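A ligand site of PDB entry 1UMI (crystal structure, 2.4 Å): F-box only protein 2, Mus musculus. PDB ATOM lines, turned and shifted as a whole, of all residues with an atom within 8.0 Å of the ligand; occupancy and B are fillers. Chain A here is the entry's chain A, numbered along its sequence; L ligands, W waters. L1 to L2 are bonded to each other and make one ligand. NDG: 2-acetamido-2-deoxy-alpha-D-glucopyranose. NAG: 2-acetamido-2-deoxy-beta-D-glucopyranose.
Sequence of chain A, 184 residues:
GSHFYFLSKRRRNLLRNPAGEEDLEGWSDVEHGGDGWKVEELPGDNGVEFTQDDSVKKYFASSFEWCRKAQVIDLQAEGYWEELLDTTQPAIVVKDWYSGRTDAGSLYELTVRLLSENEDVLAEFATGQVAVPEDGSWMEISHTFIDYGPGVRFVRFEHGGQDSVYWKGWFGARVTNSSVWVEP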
ATOM      1  N   GLY A  34       5.069  22.734  27.741  1.00  0.00           N
ATOM      2  CA  GLY A  34       4.923  22.808  26.302  1.00  0.00           C
ATOM      3  C   GLY A  34       5.166  24.197  25.819  1.00  0.00           C
ATOM      4  O   GLY A  34       6.216  24.698  26.083  1.00  0.00           O
ATOM      5  N   ASP A  35       4.248  24.824  25.107  1.00  0.00           N
ATOM      6  CA  ASP A  35       4.402  26.255  24.605  1.00  0.00           C
ATOM      7  C   ASP A  35       3.906  27.366  25.569  1.00  0.00           C
ATOM      8  O   ASP A  35       3.857  28.511  25.201  1.00  0.00           O
ATOM      9  CB  ASP A  35       3.714  26.404  23.248  1.00  0.00           C
ATOM     10  CG  ASP A  35       4.279  25.439  22.194  1.00  0.00           C
ATOM     11  OD1 ASP A  35       5.545  25.412  21.988  1.00  0.00           O
ATOM     12  OD2 ASP A  35       3.559  24.587  21.528  1.00  0.00           O
ATOM     13  N   SER A  63      -1.265  24.659  26.914  1.00  0.00           N
ATOM     14  CA  SER A  63      -0.622  24.055  25.796  1.00  0.00           C
ATOM     15  C   SER A  63      -0.530  22.520  25.992  1.00  0.00           C
ATOM     16  O   SER A  63      -1.434  21.901  26.508  1.00  0.00           O
ATOM     17  CB  SER A  63       0.741  24.675  25.606  1.00  0.00           C
ATOM     18  OG  SER A  63       1.473  24.242  24.448  1.00  0.00           O
ATOM     19  N   PHE A  64       0.527  21.899  25.541  1.00  0.00           N
ATOM     20  CA  PHE A  64       0.517  20.441  25.361  1.00  0.00           C
ATOM     21  C   PHE A  64       1.112  19.689  26.549  1.00  0.00           C
ATOM     22  O   PHE A  64       1.064  18.522  26.512  1.00  0.00           O
ATOM     23  CB  PHE A  64       1.158  20.026  24.009  1.00  0.00           C
ATOM     24  CG  PHE A  64       2.685  20.360  23.868  1.00  0.00           C
ATOM     25  CD1 PHE A  64       3.644  19.506  24.343  1.00  0.00           C
ATOM     26  CD2 PHE A  64       3.089  21.477  23.184  1.00  0.00           C
ATOM     27  CE1 PHE A  64       5.059  19.791  24.230  1.00  0.00           C
ATOM     28  CE2 PHE A  64       4.547  21.807  22.978  1.00  0.00           C
ATOM     29  CZ  PHE A  64       5.492  20.957  23.502  1.00  0.00           C
ATOM     30  N   GLU A  65       1.496  20.351  27.594  1.00  0.00           N
ATOM     31  CA  GLU A  65       1.892  19.731  28.831  1.00  0.00           C
ATOM     32  C   GLU A  65       1.336  20.686  29.965  1.00  0.00           C
ATOM     33  O   GLU A  65       0.899  21.753  29.619  1.00  0.00           O
ATOM     34  CB  GLU A  65       3.450  19.543  28.998  1.00  0.00           C
ATOM     35  CG  GLU A  65       4.006  18.432  28.097  1.00  0.00           C
ATOM     36  CD  GLU A  65       5.540  18.517  27.891  1.00  0.00           C
ATOM     37  OE1 GLU A  65       6.175  19.487  28.386  1.00  0.00           O
ATOM     38  OE2 GLU A  65       6.066  17.635  27.198  1.00  0.00           O
ATOM     39  N   ASP A 103     -12.205  21.298  18.666  1.00  0.00           N
ATOM     40  CA  ASP A 103     -11.440  20.449  17.683  1.00  0.00           C
ATOM     41  C   ASP A 103     -10.409  19.616  18.462  1.00  0.00           C
ATOM     42  O   ASP A 103      -9.559  18.874  17.908  1.00  0.00           O
ATOM     43  CB  ASP A 103     -10.732  21.326  16.555  1.00  0.00           C
ATOM     44  CG  ASP A 103      -9.955  22.543  17.099  1.00  0.00           C
ATOM     45  OD1 ASP A 103      -9.893  22.882  18.344  1.00  0.00           O
ATOM     46  OD2 ASP A 103      -9.320  23.299  16.329  1.00  0.00           O
ATOM     47  N   ALA A 104     -10.502  19.694  19.777  1.00  0.00           N
ATOM     48  CA  ALA A 104      -9.549  18.977  20.632  1.00  0.00           C
ATOM     49  C   ALA A 104      -9.910  19.099  22.088  1.00  0.00           C
ATOM     50  O   ALA A 104     -10.450  20.149  22.530  1.00  0.00           O
ATOM     51  CB  ALA A 104      -8.091  19.542  20.423  1.00  0.00           C
ATOM     52  N   ASP A 163      -3.680  20.101  27.031  1.00  0.00           N
ATOM     53  CA  ASP A 163      -4.525  19.497  26.068  1.00  0.00           C
ATOM     54  C   ASP A 163      -4.618  17.953  26.201  1.00  0.00           C
ATOM     55  O   ASP A 163      -3.967  17.218  27.041  1.00  0.00           O
ATOM     56  CB  ASP A 163      -4.166  19.969  24.639  1.00  0.00           C
ATOM     57  CG  ASP A 163      -2.882  19.404  24.134  1.00  0.00           C
ATOM     58  OD1 ASP A 163      -2.372  18.301  24.559  1.00  0.00           O
ATOM     59  OD2 ASP A 163      -2.286  20.100  23.303  1.00  0.00           O
ATOM     60  N   VAL A 165      -4.496  16.142  23.139  1.00  0.00           N
ATOM     61  CA  VAL A 165      -4.066  15.624  21.848  1.00  0.00           C
ATOM     62  C   VAL A 165      -2.506  15.720  21.675  1.00  0.00           C
ATOM     63  O   VAL A 165      -2.019  15.252  20.752  1.00  0.00           O
ATOM     64  CB  VAL A 165      -4.703  16.339  20.686  1.00  0.00           C
ATOM     65  CG1 VAL A 165      -6.150  15.705  20.396  1.00  0.00           C
ATOM     66  CG2 VAL A 165      -4.703  17.837  20.979  1.00  0.00           C
ATOM     67  N   TYR A 166      -1.786  16.356  22.595  1.00  0.00           N
ATOM     68  CA  TYR A 166      -0.333  16.618  22.507  1.00  0.00           C
ATOM     69  C   TYR A 166       0.033  17.355  21.173  1.00  0.00           C
ATOM     70  O   TYR A 166       0.779  16.837  20.301  1.00  0.00           O
ATOM     71  CB  TYR A 166       0.453  15.322  22.660  1.00  0.00           C
ATOM     72  CG  TYR A 166       1.838  15.542  23.098  1.00  0.00           C
ATOM     73  CD1 TYR A 166       2.110  15.703  24.396  1.00  0.00           C
ATOM     74  CD2 TYR A 166       2.904  15.560  22.201  1.00  0.00           C
ATOM     75  CE1 TYR A 166       3.418  15.993  24.819  1.00  0.00           C
ATOM     76  CE2 TYR A 166       4.357  15.733  22.688  1.00  0.00           C
ATOM     77  CZ  TYR A 166       4.530  15.990  24.001  1.00  0.00           C
ATOM     78  OH  TYR A 166       5.727  16.199  24.656  1.00  0.00           O
ATOM     79  N   TRP A 167      -0.532  18.567  21.044  1.00  0.00           N
ATOM     80  CA  TRP A 167      -0.470  19.445  19.844  1.00  0.00           C
ATOM     81  C   TRP A 167       0.405  20.742  20.048  1.00  0.00           C
ATOM     82  O   TRP A 167       0.273  21.445  21.095  1.00  0.00           O
ATOM     83  CB  TRP A 167      -1.902  19.775  19.386  1.00  0.00           C
ATOM     84  CG  TRP A 167      -2.546  18.708  18.537  1.00  0.00           C
ATOM     85  CD1 TRP A 167      -2.046  17.413  18.276  1.00  0.00           C
ATOM     86  CD2 TRP A 167      -3.798  18.814  17.811  1.00  0.00           C
ATOM     87  NE1 TRP A 167      -2.909  16.749  17.437  1.00  0.00           N
ATOM     88  CE2 TRP A 167      -4.002  17.561  17.145  1.00  0.00           C
ATOM     89  CE3 TRP A 167      -4.797  19.775  17.732  1.00  0.00           C
ATOM     90  CZ2 TRP A 167      -5.170  17.300  16.331  1.00  0.00           C
ATOM     91  CZ3 TRP A 167      -5.997  19.485  16.901  1.00  0.00           C
ATOM     92  CH2 TRP A 167      -6.092  18.293  16.180  1.00  0.00           C
ATOM     93  N   LYS A 168       1.389  20.989  19.146  1.00  0.00           N
ATOM     94  CA  LYS A 168       2.146  22.287  19.168  1.00  0.00           C
ATOM     95  C   LYS A 168       1.070  23.345  19.258  1.00  0.00           C
ATOM     96  O   LYS A 168       0.021  23.224  18.643  1.00  0.00           O
ATOM     97  CB  LYS A 168       3.295  22.429  18.085  1.00  0.00           C
ATOM     98  CG  LYS A 168       4.984  22.149  18.764  1.00  0.00           C
ATOM     99  CD  LYS A 168       6.078  23.421  18.833  1.00  0.00           C
ATOM    100  CE  LYS A 168       7.320  23.474  20.029  1.00  0.00           C
ATOM    101  NZ  LYS A 168       8.170  22.051  20.780  1.00  0.00           N
ATOM    102  N   GLY A 169       1.231  24.328  20.135  1.00  0.00           N
ATOM    103  CA  GLY A 169       0.169  25.347  20.228  1.00  0.00           C
ATOM    104  C   GLY A 169      -0.674  25.449  21.499  1.00  0.00           C
ATOM    105  O   GLY A 169      -0.208  25.125  22.629  1.00  0.00           O
ATOM    106  N   TRP A 170      -1.853  26.031  21.354  1.00  0.00           N
ATOM    107  CA  TRP A 170      -2.640  26.315  22.552  1.00  0.00           C
ATOM    108  C   TRP A 170      -4.038  25.558  22.536  1.00  0.00           C
ATOM    109  O   TRP A 170      -5.070  26.145  22.394  1.00  0.00           O
ATOM    110  CB  TRP A 170      -2.689  27.871  22.774  1.00  0.00           C
ATOM    111  CG  TRP A 170      -1.320  28.322  23.154  1.00  0.00           C
ATOM    112  CD1 TRP A 170      -0.738  28.225  24.390  1.00  0.00           C
ATOM    113  CD2 TRP A 170      -0.269  28.801  22.240  1.00  0.00           C
ATOM    114  NE1 TRP A 170       0.564  28.670  24.322  1.00  0.00           N
ATOM    115  CE2 TRP A 170       0.876  28.988  23.000  1.00  0.00           C
ATOM    116  CE3 TRP A 170      -0.258  29.196  20.882  1.00  0.00           C
ATOM    117  CZ2 TRP A 170       2.087  29.648  22.438  1.00  0.00           C
ATOM    118  CZ3 TRP A 170       0.912  29.757  20.336  1.00  0.00           C
ATOM    119  CH2 TRP A 170       2.068  30.024  21.145  1.00  0.00           C
ATOM    120  N   PHE A 171      -4.043  24.252  22.798  1.00  0.00           N
ATOM    121  CA  PHE A 171      -5.210  23.437  22.639  1.00  0.00           C
ATOM    122  C   PHE A 171      -5.787  22.935  23.976  1.00  0.00           C
ATOM    123  O   PHE A 171      -6.803  22.240  23.964  1.00  0.00           O
ATOM    124  CB  PHE A 171      -4.882  22.298  21.633  1.00  0.00           C
ATOM    125  CG  PHE A 171      -4.733  22.774  20.134  1.00  0.00           C
ATOM    126  CD1 PHE A 171      -5.830  22.962  19.343  1.00  0.00           C
ATOM    127  CD2 PHE A 171      -3.540  22.950  19.559  1.00  0.00           C
ATOM    128  CE1 PHE A 171      -5.767  23.323  18.027  1.00  0.00           C
ATOM    129  CE2 PHE A 171      -3.413  23.400  18.246  1.00  0.00           C
ATOM    130  CZ  PHE A 171      -4.596  23.562  17.460  1.00  0.00           C
HETATM  131  C1  NDG L   1       3.721  16.028  17.264  1.00  0.00           C
HETATM  132  C2  NDG L   1       3.067  17.394  17.549  1.00  0.00           C
HETATM  133  C3  NDG L   1       1.695  17.680  17.042  1.00  0.00           C
HETATM  134  C4  NDG L   1       1.370  17.021  15.697  1.00  0.00           C
HETATM  135  C5  NDG L   1       2.162  15.747  15.587  1.00  0.00           C
HETATM  136  C6  NDG L   1       1.719  14.874  14.485  1.00  0.00           C
HETATM  137  C7  NDG L   1       4.324  18.517  19.396  1.00  0.00           C
HETATM  138  C8  NDG L   1       4.154  18.720  20.922  1.00  0.00           C
HETATM  139  O5  NDG L   1       3.480  15.600  15.975  1.00  0.00           O
HETATM  140  O3  NDG L   1       1.412  19.022  17.122  1.00  0.00           O
HETATM  141  O4  NDG L   1      -0.045  16.922  15.394  1.00  0.00           O
HETATM  142  O6  NDG L   1       2.558  14.420  13.640  1.00  0.00           O
HETATM  143  O7  NDG L   1       5.343  18.817  18.856  1.00  0.00           O
HETATM  144  N2  NDG L   1       3.236  17.923  18.899  1.00  0.00           N
HETATM  145  O1  NDG L   1       2.838  15.040  18.057  1.00  0.00           O
HETATM  146  C1  NAG L   2      -0.533  17.996  14.588  1.00  0.00           C
HETATM  147  C2  NAG L   2      -1.695  17.706  13.668  1.00  0.00           C
HETATM  148  C3  NAG L   2      -2.448  18.841  13.018  1.00  0.00           C
HETATM  149  C4  NAG L   2      -2.626  20.089  13.886  1.00  0.00           C
HETATM  150  C5  NAG L   2      -1.450  20.215  14.864  1.00  0.00           C
HETATM  151  C6  NAG L   2      -1.650  21.210  16.026  1.00  0.00           C
HETATM  152  C7  NAG L   2      -1.707  15.257  13.027  1.00  0.00           C
HETATM  153  C8  NAG L   2      -1.374  14.286  11.987  1.00  0.00           C
HETATM  154  N2  NAG L   2      -1.449  16.593  12.799  1.00  0.00           N
HETATM  155  O3  NAG L   2      -3.652  18.468  12.407  1.00  0.00           O
HETATM  156  O4  NAG L   2      -2.993  21.339  13.225  1.00  0.00           O
HETATM  157  O5  NAG L   2      -0.729  19.094  15.407  1.00  0.00           O
HETATM  158  O6  NAG L   2      -0.364  21.412  16.645  1.00  0.00           O
HETATM  159  O7  NAG L   2      -2.262  14.740  13.880  1.00  0.00           O
HETATM  160  O   HOH W   1       0.003  17.480  10.313  1.00  0.00           O
HETATM  161  O   HOH W   2      -1.465  14.477  16.662  1.00  0.00           O
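N of Lys 168 is in hydrogen-bond range of O3 of NDG L1 (2.8 Å). O of Tyr 166 lies within hydrogen-bond range of N2 of NDG L1 (3.0 Å). O6 of NAG L2 is in hydrogen-bond range of O of Lys 168, 2.7 Å away.
The backbone NH (N) of Tyr 166 lies within hydrogen-bond range of the side-chain carboxylate (OD1) of Asp 163. N of Trp 167 lies within hydrogen-bond range of OD2 of Asp 163 (3.2 Å). OH of Tyr 166 lies within hydrogen-bond range of OE2 of Glu 65 (2.9 Å).
Merely in contact with the ligand: Trp 167 (3.3 Å), Phe 64 (3.5 Å) and Phe 171 (3.6 Å). Hydrophobic or aromatic side chains that line the ligand: Phe 64, Tyr 166, Trp 167 and Phe 171. Of the 15 residues printed, 5 come within 4 Å of the ligand. Along chain A the residues within 4 Å of the ligand span positions 64 to 171.
Water W2 bridges the indole nitrogen (NE1) of Trp 167 and an oxygen (O7) of NAG L2.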
